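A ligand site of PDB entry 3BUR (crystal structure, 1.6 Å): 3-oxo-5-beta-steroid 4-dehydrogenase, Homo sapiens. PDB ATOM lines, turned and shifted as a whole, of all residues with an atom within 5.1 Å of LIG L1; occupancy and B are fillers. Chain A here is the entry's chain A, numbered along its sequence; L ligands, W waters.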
ATOM      1  N   GLY A  24     -12.610  25.215  18.812  1.00  0.00           N
ATOM      2  CA  GLY A  24     -13.921  25.846  18.870  1.00  0.00           C
ATOM      3  C   GLY A  24     -14.042  26.643  20.150  1.00  0.00           C
ATOM      4  O   GLY A  24     -13.397  26.317  21.158  1.00  0.00           O
ATOM      5  N   THR A  25     -14.848  27.724  20.147  1.00  0.00           N
ATOM      6  CA  THR A  25     -14.865  28.556  21.341  1.00  0.00           C
ATOM      7  C   THR A  25     -16.258  28.863  21.884  1.00  0.00           C
ATOM      8  O   THR A  25     -16.430  29.765  22.703  1.00  0.00           O
ATOM      9  CB  THR A  25     -14.134  29.897  21.091  1.00  0.00           C
ATOM     10  OG1 THR A  25     -14.762  30.579  19.993  1.00  0.00           O
ATOM     11  CG2 THR A  25     -12.682  29.645  20.711  1.00  0.00           C
ATOM     12  N   TYR A  26     -17.297  28.128  21.456  1.00  0.00           N
ATOM     13  CA  TYR A  26     -18.595  28.369  22.060  1.00  0.00           C
ATOM     14  C   TYR A  26     -18.519  27.795  23.487  1.00  0.00           C
ATOM     15  O   TYR A  26     -18.113  26.664  23.694  1.00  0.00           O
ATOM     16  CB  TYR A  26     -19.794  27.741  21.330  1.00  0.00           C
ATOM     17  CG  TYR A  26     -21.052  27.845  22.188  1.00  0.00           C
ATOM     18  CD1 TYR A  26     -21.740  29.052  22.266  1.00  0.00           C
ATOM     19  CD2 TYR A  26     -21.563  26.766  22.919  1.00  0.00           C
ATOM     20  CE1 TYR A  26     -22.876  29.119  23.051  1.00  0.00           C
ATOM     21  CE2 TYR A  26     -22.691  26.842  23.710  1.00  0.00           C
ATOM     22  CZ  TYR A  26     -23.349  28.046  23.765  1.00  0.00           C
ATOM     23  OH  TYR A  26     -24.471  28.126  24.537  1.00  0.00           O
ATOM     24  N   ASP A  53     -11.911  29.045  15.958  1.00  0.00           N
ATOM     25  CA  ASP A  53     -13.244  29.291  15.459  1.00  0.00           C
ATOM     26  C   ASP A  53     -14.069  29.994  16.515  1.00  0.00           C
ATOM     27  O   ASP A  53     -14.193  29.515  17.632  1.00  0.00           O
ATOM     28  CB  ASP A  53     -13.951  27.978  15.042  1.00  0.00           C
ATOM     29  CG  ASP A  53     -15.312  28.328  14.469  1.00  0.00           C
ATOM     30  OD1 ASP A  53     -15.391  28.654  13.269  1.00  0.00           O
ATOM     31  OD2 ASP A  53     -16.280  28.304  15.261  1.00  0.00           O
ATOM     32  N   GLY A  54     -14.626  31.161  16.164  1.00  0.00           N
ATOM     33  CA  GLY A  54     -15.367  31.950  17.127  1.00  0.00           C
ATOM     34  C   GLY A  54     -16.546  32.681  16.507  1.00  0.00           C
ATOM     35  O   GLY A  54     -16.896  32.468  15.342  1.00  0.00           O
ATOM     36  N   TYR A  58     -20.982  34.441  20.522  1.00  0.00           N
ATOM     37  CA  TYR A  58     -20.571  33.550  21.607  1.00  0.00           C
ATOM     38  C   TYR A  58     -20.216  34.375  22.832  1.00  0.00           C
ATOM     39  O   TYR A  58     -20.005  33.797  23.905  1.00  0.00           O
ATOM     40  CB  TYR A  58     -19.388  32.648  21.261  1.00  0.00           C
ATOM     41  CG  TYR A  58     -19.605  31.746  20.067  1.00  0.00           C
ATOM     42  CD1 TYR A  58     -20.857  31.572  19.504  1.00  0.00           C
ATOM     43  CD2 TYR A  58     -18.535  31.063  19.491  1.00  0.00           C
ATOM     44  CE1 TYR A  58     -21.074  30.745  18.402  1.00  0.00           C
ATOM     45  CE2 TYR A  58     -18.756  30.244  18.401  1.00  0.00           C
ATOM     46  CZ  TYR A  58     -20.004  30.087  17.854  1.00  0.00           C
ATOM     47  OH  TYR A  58     -20.171  29.263  16.759  1.00  0.00           O
ATOM     48  N   LYS A  87     -18.218  35.032  12.455  1.00  0.00           N
ATOM     49  CA  LYS A  87     -19.496  34.710  11.850  1.00  0.00           C
ATOM     50  C   LYS A  87     -20.494  35.861  11.937  1.00  0.00           C
ATOM     51  O   LYS A  87     -20.609  36.590  12.933  1.00  0.00           O
ATOM     52  CB  LYS A  87     -20.137  33.477  12.534  1.00  0.00           C
ATOM     53  CG  LYS A  87     -19.205  32.283  12.696  1.00  0.00           C
ATOM     54  CD  LYS A  87     -19.901  30.985  13.055  1.00  0.00           C
ATOM     55  CE  LYS A  87     -18.892  29.863  13.357  1.00  0.00           C
ATOM     56  NZ  LYS A  87     -18.268  30.041  14.708  1.00  0.00           N
ATOM     57  N   GLU A 120     -23.631  32.909   9.379  1.00  0.00           N
ATOM     58  CA  GLU A 120     -23.699  31.973  10.502  1.00  0.00           C
ATOM     59  C   GLU A 120     -24.810  30.918  10.379  1.00  0.00           C
ATOM     60  O   GLU A 120     -24.651  29.733  10.716  1.00  0.00           O
ATOM     61  CB  GLU A 120     -23.895  32.747  11.815  1.00  0.00           C
ATOM     62  CG  GLU A 120     -23.612  31.878  13.055  1.00  0.00           C
ATOM     63  CD  GLU A 120     -23.144  32.731  14.228  1.00  0.00           C
ATOM     64  OE1 GLU A 120     -23.264  33.973  14.199  1.00  0.00           O
ATOM     65  OE2 GLU A 120     -22.650  32.171  15.220  1.00  0.00           O
ATOM     66  N   VAL A 121     -25.962  31.363   9.933  1.00  0.00           N
ATOM     67  CA  VAL A 121     -27.084  30.550   9.502  1.00  0.00           C
ATOM     68  C   VAL A 121     -27.710  31.180   8.252  1.00  0.00           C
ATOM     69  O   VAL A 121     -27.567  32.394   8.049  1.00  0.00           O
ATOM     70  CB  VAL A 121     -28.138  30.430  10.600  1.00  0.00           C
ATOM     71  CG1 VAL A 121     -27.613  29.541  11.724  1.00  0.00           C
ATOM     72  CG2 VAL A 121     -28.566  31.794  11.139  1.00  0.00           C
ATOM     73  N   SER A 169     -22.408  28.868   6.670  1.00  0.00           N
ATOM     74  CA  SER A 169     -22.595  27.856   7.713  1.00  0.00           C
ATOM     75  C   SER A 169     -24.064  27.448   7.801  1.00  0.00           C
ATOM     76  O   SER A 169     -24.941  28.316   7.706  1.00  0.00           O
ATOM     77  CB  SER A 169     -22.056  28.433   9.024  1.00  0.00           C
ATOM     78  OG  SER A 169     -22.247  27.512  10.075  1.00  0.00           O
ATOM     79  N   ASN A 170     -24.299  26.146   7.996  1.00  0.00           N
ATOM     80  CA  ASN A 170     -25.638  25.574   8.083  1.00  0.00           C
ATOM     81  C   ASN A 170     -26.402  25.855   6.784  1.00  0.00           C
ATOM     82  O   ASN A 170     -27.612  26.060   6.871  1.00  0.00           O
ATOM     83  CB  ASN A 170     -26.390  26.187   9.264  1.00  0.00           C
ATOM     84  CG  ASN A 170     -25.714  25.815  10.576  1.00  0.00           C
ATOM     85  OD1 ASN A 170     -25.628  24.615  10.852  1.00  0.00           O
ATOM     86  ND2 ASN A 170     -25.266  26.795  11.349  1.00  0.00           N
ATOM     87  N   GLN A 193     -19.575  25.502   7.010  1.00  0.00           N
ATOM     88  CA  GLN A 193     -19.420  24.958   8.362  1.00  0.00           C
ATOM     89  C   GLN A 193     -20.720  24.304   8.791  1.00  0.00           C
ATOM     90  O   GLN A 193     -21.735  24.988   8.911  1.00  0.00           O
ATOM     91  CB  GLN A 193     -18.997  26.037   9.354  1.00  0.00           C
ATOM     92  CG  GLN A 193     -18.594  25.403  10.697  1.00  0.00           C
ATOM     93  CD  GLN A 193     -18.178  26.446  11.710  1.00  0.00           C
ATOM     94  OE1 GLN A 193     -18.814  26.645  12.754  1.00  0.00           O
ATOM     95  NE2 GLN A 193     -17.077  27.164  11.453  1.00  0.00           N
ATOM     96  N   TYR A 219     -18.452  21.465  12.491  1.00  0.00           N
ATOM     97  CA  TYR A 219     -18.733  21.928  13.846  1.00  0.00           C
ATOM     98  C   TYR A 219     -19.260  20.731  14.654  1.00  0.00           C
ATOM     99  O   TYR A 219     -19.621  19.714  14.056  1.00  0.00           O
ATOM    100  CB  TYR A 219     -19.663  23.119  13.858  1.00  0.00           C
ATOM    101  CG  TYR A 219     -21.143  23.131  13.666  1.00  0.00           C
ATOM    102  CD1 TYR A 219     -22.048  22.455  14.478  1.00  0.00           C
ATOM    103  CD2 TYR A 219     -21.733  23.874  12.638  1.00  0.00           C
ATOM    104  CE1 TYR A 219     -23.419  22.472  14.304  1.00  0.00           C
ATOM    105  CE2 TYR A 219     -23.105  23.927  12.439  1.00  0.00           C
ATOM    106  CZ  TYR A 219     -23.945  23.220  13.278  1.00  0.00           C
ATOM    107  OH  TYR A 219     -25.313  23.243  13.128  1.00  0.00           O
ATOM    108  N   SER A 220     -19.312  20.893  15.970  1.00  0.00           N
ATOM    109  CA  SER A 220     -19.636  19.801  16.894  1.00  0.00           C
ATOM    110  C   SER A 220     -19.011  18.469  16.485  1.00  0.00           C
ATOM    111  O   SER A 220     -19.714  17.448  16.404  1.00  0.00           O
ATOM    112  CB  SER A 220     -21.156  19.692  16.997  1.00  0.00           C
ATOM    113  OG  SER A 220     -21.702  20.942  17.394  1.00  0.00           O
ATOM    114  N   PRO A 221     -17.711  18.432  16.197  1.00  0.00           N
ATOM    115  CA  PRO A 221     -17.103  17.215  15.655  1.00  0.00           C
ATOM    116  C   PRO A 221     -16.967  16.114  16.716  1.00  0.00           C
ATOM    117  O   PRO A 221     -16.661  14.969  16.367  1.00  0.00           O
ATOM    118  CB  PRO A 221     -15.698  17.683  15.233  1.00  0.00           C
ATOM    119  CG  PRO A 221     -15.401  18.825  16.161  1.00  0.00           C
ATOM    120  CD  PRO A 221     -16.701  19.521  16.367  1.00  0.00           C
ATOM    121  N   LEU A 222     -17.207  16.480  17.957  1.00  0.00           N
ATOM    122  CA  LEU A 222     -17.234  15.476  19.026  1.00  0.00           C
ATOM    123  C   LEU A 222     -18.663  15.226  19.477  1.00  0.00           C
ATOM    124  O   LEU A 222     -18.900  14.592  20.499  1.00  0.00           O
ATOM    125  CB  LEU A 222     -16.445  15.913  20.264  1.00  0.00           C
ATOM    126  CG  LEU A 222     -14.994  16.326  19.986  1.00  0.00           C
ATOM    127  CD1 LEU A 222     -14.310  16.744  21.281  1.00  0.00           C
ATOM    128  CD2 LEU A 222     -14.275  15.175  19.304  1.00  0.00           C
ATOM    129  N   GLY A 223     -19.640  15.724  18.714  1.00  0.00           N
ATOM    130  CA  GLY A 223     -21.012  15.350  19.038  1.00  0.00           C
ATOM    131  C   GLY A 223     -21.733  16.315  19.939  1.00  0.00           C
ATOM    132  O   GLY A 223     -22.830  15.994  20.415  1.00  0.00           O
ATOM    133  N   THR A 224     -21.189  17.494  20.193  1.00  0.00           N
ATOM    134  CA  THR A 224     -21.722  18.571  21.011  1.00  0.00           C
ATOM    135  C   THR A 224     -21.529  18.318  22.516  1.00  0.00           C
ATOM    136  O   THR A 224     -21.237  17.220  22.984  1.00  0.00           O
ATOM    137  CB  THR A 224     -23.216  18.924  20.847  1.00  0.00           C
ATOM    138  OG1 THR A 224     -24.052  17.961  21.533  1.00  0.00           O
ATOM    139  CG2 THR A 224     -23.701  18.899  19.395  1.00  0.00           C
ATOM    140  N   SER A 225     -21.733  19.420  23.239  1.00  0.00           N
ATOM    141  CA  SER A 225     -21.760  19.372  24.701  1.00  0.00           C
ATOM    142  C   SER A 225     -23.087  18.803  25.204  1.00  0.00           C
ATOM    143  O   SER A 225     -23.296  18.628  26.402  1.00  0.00           O
ATOM    144  CB  SER A 225     -21.525  20.775  25.254  1.00  0.00           C
ATOM    145  OG  SER A 225     -22.676  21.570  25.003  1.00  0.00           O
ATOM    146  N   LEU A 239     -19.378   9.773  21.946  1.00  0.00           N
ATOM    147  CA  LEU A 239     -18.078   9.354  22.483  1.00  0.00           C
ATOM    148  C   LEU A 239     -18.230   8.065  23.283  1.00  0.00           C
ATOM    149  O   LEU A 239     -17.223   7.563  23.753  1.00  0.00           O
ATOM    150  CB  LEU A 239     -17.437  10.461  23.308  1.00  0.00           C
ATOM    151  CG  LEU A 239     -17.101  11.737  22.494  1.00  0.00           C
ATOM    152  CD1 LEU A 239     -16.454  12.779  23.393  1.00  0.00           C
ATOM    153  CD2 LEU A 239     -16.239  11.401  21.294  1.00  0.00           C
ATOM    154  N   THR A 254      -8.287   7.967  22.547  1.00  0.00           N
ATOM    155  CA  THR A 254      -9.638   8.010  23.100  1.00  0.00           C
ATOM    156  C   THR A 254     -10.639   8.011  21.938  1.00  0.00           C
ATOM    157  O   THR A 254     -10.184   8.220  20.823  1.00  0.00           O
ATOM    158  CB  THR A 254      -9.895   9.279  23.938  1.00  0.00           C
ATOM    159  OG1 THR A 254      -9.626  10.434  23.138  1.00  0.00           O
ATOM    160  CG2 THR A 254      -8.950   9.328  25.134  1.00  0.00           C
ATOM    161  N   ALA A 256     -12.622  10.298  21.236  1.00  0.00           N
ATOM    162  CA  ALA A 256     -12.542  11.654  20.696  1.00  0.00           C
ATOM    163  C   ALA A 256     -11.455  11.751  19.627  1.00  0.00           C
ATOM    164  O   ALA A 256     -11.596  12.276  18.535  1.00  0.00           O
ATOM    165  CB  ALA A 256     -12.270  12.634  21.818  1.00  0.00           C
ATOM    166  N   ILE A 271     -13.243  21.391  14.321  1.00  0.00           N
ATOM    167  CA  ILE A 271     -13.025  22.467  15.293  1.00  0.00           C
ATOM    168  C   ILE A 271     -13.569  22.141  16.665  1.00  0.00           C
ATOM    169  O   ILE A 271     -14.425  22.811  17.237  1.00  0.00           O
ATOM    170  CB  ILE A 271     -13.690  23.767  14.794  1.00  0.00           C
ATOM    171  CG1 ILE A 271     -15.142  23.611  14.316  1.00  0.00           C
ATOM    172  CG2 ILE A 271     -12.796  24.336  13.684  1.00  0.00           C
ATOM    173  CD1 ILE A 271     -15.838  24.945  14.051  1.00  0.00           C
ATOM    174  N   PRO A 272     -12.987  21.085  17.243  1.00  0.00           N
ATOM    175  CA  PRO A 272     -13.496  20.651  18.549  1.00  0.00           C
ATOM    176  C   PRO A 272     -13.265  21.739  19.573  1.00  0.00           C
ATOM    177  O   PRO A 272     -12.225  22.427  19.611  1.00  0.00           O
ATOM    178  CB  PRO A 272     -12.648  19.423  18.858  1.00  0.00           C
ATOM    179  CG  PRO A 272     -11.391  19.625  18.055  1.00  0.00           C
ATOM    180  CD  PRO A 272     -11.852  20.292  16.785  1.00  0.00           C
ATOM    181  N   LYS A 273     -14.238  21.921  20.462  1.00  0.00           N
ATOM    182  CA  LYS A 273     -14.109  22.879  21.540  1.00  0.00           C
ATOM    183  C   LYS A 273     -13.681  22.137  22.814  1.00  0.00           C
ATOM    184  O   LYS A 273     -14.351  21.170  23.212  1.00  0.00           O
ATOM    185  CB  LYS A 273     -15.421  23.627  21.839  1.00  0.00           C
ATOM    186  CG  LYS A 273     -15.384  24.539  23.059  1.00  0.00           C
ATOM    187  CD  LYS A 273     -16.024  23.885  24.292  1.00  0.00           C
ATOM    188  CE  LYS A 273     -15.885  24.783  25.523  1.00  0.00           C
ATOM    189  NZ  LYS A 273     -16.343  24.072  26.754  1.00  0.00           N
ATOM    190  N   SER A 274     -12.665  22.653  23.467  1.00  0.00           N
ATOM    191  CA  SER A 274     -12.431  22.261  24.859  1.00  0.00           C
ATOM    192  C   SER A 274     -11.895  23.460  25.646  1.00  0.00           C
ATOM    193  O   SER A 274     -11.036  24.160  25.116  1.00  0.00           O
ATOM    194  CB  SER A 274     -11.455  21.084  24.954  1.00  0.00           C
ATOM    195  OG  SER A 274     -11.211  20.867  26.344  1.00  0.00           O
ATOM    196  N   PHE A 275     -12.370  23.709  26.865  1.00  0.00           N
ATOM    197  CA  PHE A 275     -11.718  24.715  27.693  1.00  0.00           C
ATOM    198  C   PHE A 275     -10.967  24.015  28.830  1.00  0.00           C
ATOM    199  O   PHE A 275     -10.705  24.611  29.875  1.00  0.00           O
ATOM    200  CB  PHE A 275     -12.697  25.759  28.239  1.00  0.00           C
ATOM    201  CG  PHE A 275     -13.161  26.778  27.207  1.00  0.00           C
ATOM    202  CD1 PHE A 275     -14.064  27.760  27.572  1.00  0.00           C
ATOM    203  CD2 PHE A 275     -12.678  26.750  25.899  1.00  0.00           C
ATOM    204  CE1 PHE A 275     -14.480  28.701  26.648  1.00  0.00           C
ATOM    205  CE2 PHE A 275     -13.112  27.682  24.967  1.00  0.00           C
ATOM    206  CZ  PHE A 275     -14.008  28.652  25.342  1.00  0.00           C
ATOM    207  N   ASN A 276     -10.640  22.756  28.604  1.00  0.00           N
ATOM    208  CA  ASN A 276      -9.931  21.958  29.597  1.00  0.00           C
ATOM    209  C   ASN A 276      -8.515  21.745  29.105  1.00  0.00           C
ATOM    210  O   ASN A 276      -8.312  21.246  28.006  1.00  0.00           O
ATOM    211  CB  ASN A 276     -10.648  20.621  29.777  1.00  0.00           C
ATOM    212  CG  ASN A 276      -9.878  19.729  30.749  1.00  0.00           C
ATOM    213  OD1 ASN A 276      -8.907  19.073  30.361  1.00  0.00           O
ATOM    214  ND2 ASN A 276     -10.329  19.719  31.996  1.00  0.00           N
ATOM    215  N   ARG A 279      -7.749  18.145  27.739  1.00  0.00           N
ATOM    216  CA  ARG A 279      -8.487  17.736  26.536  1.00  0.00           C
ATOM    217  C   ARG A 279      -8.099  18.582  25.321  1.00  0.00           C
ATOM    218  O   ARG A 279      -8.122  18.091  24.198  1.00  0.00           O
ATOM    219  CB  ARG A 279      -9.993  17.811  26.804  1.00  0.00           C
ATOM    220  CG  ARG A 279     -10.464  16.689  27.723  1.00  0.00           C
ATOM    221  CD  ARG A 279     -11.955  16.599  27.896  1.00  0.00           C
ATOM    222  NE  ARG A 279     -12.517  17.620  28.734  1.00  0.00           N
ATOM    223  CZ  ARG A 279     -12.522  17.659  30.072  1.00  0.00           C
ATOM    224  NH1 ARG A 279     -11.961  16.671  30.766  1.00  0.00           N
ATOM    225  NH2 ARG A 279     -13.101  18.680  30.688  1.00  0.00           N
ATOM    226  N   GLU A 282      -5.195  16.669  24.241  1.00  0.00           N
ATOM    227  CA  GLU A 282      -5.622  15.367  23.719  1.00  0.00           C
ATOM    228  C   GLU A 282      -6.160  15.496  22.293  1.00  0.00           C
ATOM    229  O   GLU A 282      -5.809  14.722  21.413  1.00  0.00           O
ATOM    230  CB  GLU A 282      -6.694  14.778  24.643  1.00  0.00           C
ATOM    231  CG  GLU A 282      -7.309  13.484  24.111  1.00  0.00           C
ATOM    232  CD  GLU A 282      -8.486  13.079  24.995  1.00  0.00           C
ATOM    233  OE1 GLU A 282      -9.522  12.624  24.489  1.00  0.00           O
ATOM    234  OE2 GLU A 282      -8.366  13.206  26.244  1.00  0.00           O
ATOM    235  N   ASN A 283      -7.011  16.479  22.091  1.00  0.00           N
ATOM    236  CA  ASN A 283      -7.651  16.620  20.773  1.00  0.00           C
ATOM    237  C   ASN A 283      -6.662  16.980  19.673  1.00  0.00           C
ATOM    238  O   ASN A 283      -6.920  16.728  18.488  1.00  0.00           O
ATOM    239  CB  ASN A 283      -8.732  17.703  20.859  1.00  0.00           C
ATOM    240  CG  ASN A 283      -9.899  17.339  21.744  1.00  0.00           C
ATOM    241  OD1 ASN A 283     -10.122  16.174  22.082  1.00  0.00           O
ATOM    242  ND2 ASN A 283     -10.672  18.348  22.128  1.00  0.00           N
HETATM  243  P1  LIG L   1     -17.964  19.627  20.244  1.00  0.00           P
HETATM  244  O1  LIG L   1     -18.403  18.587  19.418  1.00  0.00           O
HETATM  245  O2  LIG L   1     -16.647  20.283  19.919  1.00  0.00           O
HETATM  246  O3  LIG L   1     -17.886  19.117  21.815  1.00  0.00           O
HETATM  247  C1  LIG L   1     -17.536  19.811  22.815  1.00  0.00           C
HETATM  248  C2  LIG L   1     -17.932  19.198  24.197  1.00  0.00           C
HETATM  249  O4  LIG L   1     -17.004  18.183  24.332  1.00  0.00           O
HETATM  250  C3  LIG L   1     -17.627  20.133  25.407  1.00  0.00           C
HETATM  251  O5  LIG L   1     -18.598  19.827  26.396  1.00  0.00           O
HETATM  252  C4  LIG L   1     -16.229  19.741  25.843  1.00  0.00           C
HETATM  253  O6  LIG L   1     -16.001  19.904  27.268  1.00  0.00           O
HETATM  254  C5  LIG L   1     -16.187  18.268  25.502  1.00  0.00           C
HETATM  255  N1  LIG L   1     -14.902  17.743  25.091  1.00  0.00           N
HETATM  256  C6  LIG L   1     -13.945  18.381  24.343  1.00  0.00           C
HETATM  257  N2  LIG L   1     -12.898  17.555  24.074  1.00  0.00           N
HETATM  258  C7  LIG L   1     -13.244  16.386  24.703  1.00  0.00           C
HETATM  259  C8  LIG L   1     -12.495  15.204  24.781  1.00  0.00           C
HETATM  260  N3  LIG L   1     -11.305  14.910  24.301  1.00  0.00           N
HETATM  261  N4  LIG L   1     -13.133  14.125  25.511  1.00  0.00           N
HETATM  262  C9  LIG L   1     -14.372  14.283  26.043  1.00  0.00           C
HETATM  263  N5  LIG L   1     -15.069  15.432  25.997  1.00  0.00           N
HETATM  264  C10 LIG L   1     -14.484  16.532  25.296  1.00  0.00           C
HETATM  265  O7  LIG L   1     -18.946  20.826  20.195  1.00  0.00           O
HETATM  266  P2  LIG L   1     -19.355  22.240  19.897  1.00  0.00           P
HETATM  267  O8  LIG L   1     -20.730  22.351  19.764  1.00  0.00           O
HETATM  268  O9  LIG L   1     -18.627  23.152  20.872  1.00  0.00           O
HETATM  269  O10 LIG L   1     -18.615  22.284  18.640  1.00  0.00           O
HETATM  270  C11 LIG L   1     -17.386  22.831  18.206  1.00  0.00           C
HETATM  271  C12 LIG L   1     -17.249  24.262  17.832  1.00  0.00           C
HETATM  272  O11 LIG L   1     -17.904  24.440  16.527  1.00  0.00           O
HETATM  273  C13 LIG L   1     -18.008  25.319  18.718  1.00  0.00           C
HETATM  274  O12 LIG L   1     -17.314  25.610  19.988  1.00  0.00           O
HETATM  275  C14 LIG L   1     -18.144  26.491  17.716  1.00  0.00           C
HETATM  276  O13 LIG L   1     -16.832  27.119  17.643  1.00  0.00           O
HETATM  277  C15 LIG L   1     -18.506  25.736  16.449  1.00  0.00           C
HETATM  278  N6  LIG L   1     -19.967  25.493  16.209  1.00  0.00           N
HETATM  279  C16 LIG L   1     -20.509  26.208  15.137  1.00  0.00           C
HETATM  280  C17 LIG L   1     -21.909  26.238  14.989  1.00  0.00           C
HETATM  281  C18 LIG L   1     -22.482  27.019  13.823  1.00  0.00           C
HETATM  282  O14 LIG L   1     -23.699  27.040  13.694  1.00  0.00           O
HETATM  283  N7  LIG L   1     -21.570  27.617  13.051  1.00  0.00           N
HETATM  284  C19 LIG L   1     -22.777  25.544  15.907  1.00  0.00           C
HETATM  285  C20 LIG L   1     -22.243  24.804  17.003  1.00  0.00           C
HETATM  286  C21 LIG L   1     -20.853  24.783  17.150  1.00  0.00           C
HETATM  287  P3  LIG L   1     -14.641  20.633  27.807  1.00  0.00           P
HETATM  288  O15 LIG L   1     -14.611  22.063  27.288  1.00  0.00           O
HETATM  289  O16 LIG L   1     -14.799  20.623  29.340  1.00  0.00           O
HETATM  290  O17 LIG L   1     -13.463  19.804  27.291  1.00  0.00           O
HETATM  291  C1  LG2 L   2     -25.196  24.835  22.337  1.00  0.00           C
HETATM  292  C2  LG2 L   2     -24.619  23.620  23.052  1.00  0.00           C
HETATM  293  C3  LG2 L   2     -25.036  22.364  22.349  1.00  0.00           C
HETATM  294  O1  LG2 L   2     -25.108  21.298  22.977  1.00  0.00           O
HETATM  295  C4  LG2 L   2     -25.011  22.400  20.894  1.00  0.00           C
HETATM  296  C5  LG2 L   2     -25.169  23.563  20.196  1.00  0.00           C
HETATM  297  C6  LG2 L   2     -25.307  23.528  18.722  1.00  0.00           C
HETATM  298  C7  LG2 L   2     -26.044  24.724  18.099  1.00  0.00           C
HETATM  299  C8  LG2 L   2     -25.534  26.062  18.625  1.00  0.00           C
HETATM  300  C9  LG2 L   2     -25.623  26.054  20.172  1.00  0.00           C
HETATM  301  C10 LG2 L   2     -24.799  24.907  20.848  1.00  0.00           C
HETATM  302  C11 LG2 L   2     -25.290  27.445  20.778  1.00  0.00           C
HETATM  303  C12 LG2 L   2     -26.181  28.564  20.171  1.00  0.00           C
HETATM  304  C13 LG2 L   2     -26.003  28.574  18.645  1.00  0.00           C
HETATM  305  C14 LG2 L   2     -26.424  27.194  18.108  1.00  0.00           C
HETATM  306  C15 LG2 L   2     -26.568  27.393  16.586  1.00  0.00           C
HETATM  307  C16 LG2 L   2     -26.981  28.864  16.418  1.00  0.00           C
HETATM  308  C17 LG2 L   2     -27.033  29.449  17.870  1.00  0.00           C
HETATM  309  O2  LG2 L   2     -26.698  30.840  17.838  1.00  0.00           O
HETATM  310  C18 LG2 L   2     -24.600  29.024  18.261  1.00  0.00           C
HETATM  311  C19 LG2 L   2     -23.283  25.092  20.662  1.00  0.00           C
HETATM  312  O   HOH W   1     -11.740  11.658  25.848  1.00  0.00           O
HETATM  313  O   HOH W   2     -18.906  21.423  28.542  1.00  0.00           O
HETATM  314  O   HOH W   3     -21.892  21.965  21.989  1.00  0.00           O
HETATM  315  O   HOH W   4     -14.240  22.710  30.665  1.00  0.00           O
HETATM  316  O   HOH W   5     -22.485  29.623  15.584  1.00  0.00           O
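The side-chain hydroxyl (OG) of Ser 274 sits at hydrogen-bond distance from an oxygen (O17) of LIG L1. N of Lys 273 lies within hydrogen-bond range of O2 of LIG L1. NZ of Lys 273 is in salt-bridge range of O15 of LIG L1, at 2.7 Å. The side-chain carboxylate of Asp 53 is in hydrogen-bond range of an oxygen (O13) of LIG L1, 2.7 Å away. An oxygen (O17) of LIG L1 is in salt-bridge range of the guanidinium group (NE) of Arg 279 (2.8 Å). O15 of LIG L1 lies within hydrogen-bond range of N of Phe 275, at 2.8 Å. OD1 of Asn 283 is in hydrogen-bond range of N3 of LIG L1. An oxygen (O1) of LIG L1 lies within hydrogen-bond range of the backbone NH of Leu 222, at 2.8 Å. ND2 of Asn 170 is in hydrogen-bond range of O14 of LIG L1 (2.8 Å). A nitrogen (N3) of LIG L1 is in hydrogen-bond range of the side-chain carboxylate (OE1) of Glu 282 (2.9 Å). An oxygen (O12) of LIG L1 sits at hydrogen-bond distance from the backbone NH (N) of Tyr 26 (2.9 Å). O10 of LIG L1 lies within hydrogen-bond range of N of Ser 220 (3.1 Å). The side-chain hydroxyl (OG) of Ser 220 is in hydrogen-bond range of an oxygen (O8) of LIG L1, 2.9 Å away. A nitrogen (N7) of LIG L1 is in hydrogen-bond range of the side-chain amide oxygen of Gln 193 (2.9 Å). N7 of LIG L1 lies within hydrogen-bond range of OG of Ser 169, 3.1 Å away. O1 of LIG L1 is in hydrogen-bond range of N of Thr 224, at 3.1 Å. An oxygen (O1) of LIG L1 is in hydrogen-bond range of the backbone NH of Gly 223. O12 of LIG L1 lies within hydrogen-bond range of N of Thr 25, 3.3 Å away. O1 of LG2 L2 sits at hydrogen-bond distance from OG of Ser 225 (3.2 Å).
N of Pro 221 sits close to O1 of LIG L1 (3.3 Å). Merely in contact with LIG L1: Gly 24, Tyr 58, Lys 87, Tyr 219, Ser 225, Leu 239, Ala 256, Ile 271, Pro 272 and Asn 276. Hydrophobic or aromatic side chains within 4 Å of LIG L1: Tyr 26, Tyr 58, Tyr 219, Pro 221, Leu 222, Leu 239, Ala 256 and Ile 271. Along chain A the residues within 4 Å of LIG L1 span positions 24 to 283.
Water W3 lies within hydrogen-bond range of an oxygen (O8) of LIG L1, the backbone NH (N) of Ser 225 and an oxygen (O1) of LG2 L2. Water W1 bridges the side-chain carboxylate of Glu 282 (2.8 Å) and a nitrogen (N4) of LIG L1 (2.9 Å). Water W5 lies within hydrogen-bond range of the side-chain carboxylate (OE2) of Glu 120 (2.6 Å), the side-chain hydroxyl (OH) of Tyr 58 (2.6 Å) and a nitrogen (N7) of LIG L1 (3.4 Å).
OD2 of Asp 53 is in salt-bridge range of NZ of Lys 87, 2.7 Å away. The backbone carbonyl oxygen (O) of Arg 279 sits close to the side-chain amide nitrogen (ND2) of Asn 283. The backbone NH (N) of Asn 170 sits at hydrogen-bond distance from the backbone carbonyl oxygen (O) of Gln 193 (3.0 Å). ND2 of Asn 170 lies within hydrogen-bond range of OG of Ser 169 (3.4 Å). OD1 of Asn 170 lies within hydrogen-bond range of OH of Tyr 219, at 2.7 Å. The backbone carbonyl oxygen (O) of Gln 193 is in hydrogen-bond range of the side-chain hydroxyl (OG) of Ser 169, 2.8 Å away. The backbone carbonyl oxygen (O) of Glu 120 is in hydrogen-bond range of the side-chain hydroxyl (OG) of Ser 169, at 3.3 Å. The backbone NH of Gly 24 lies within hydrogen-bond range of the backbone carbonyl oxygen of Ile 271 (3.4 Å).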
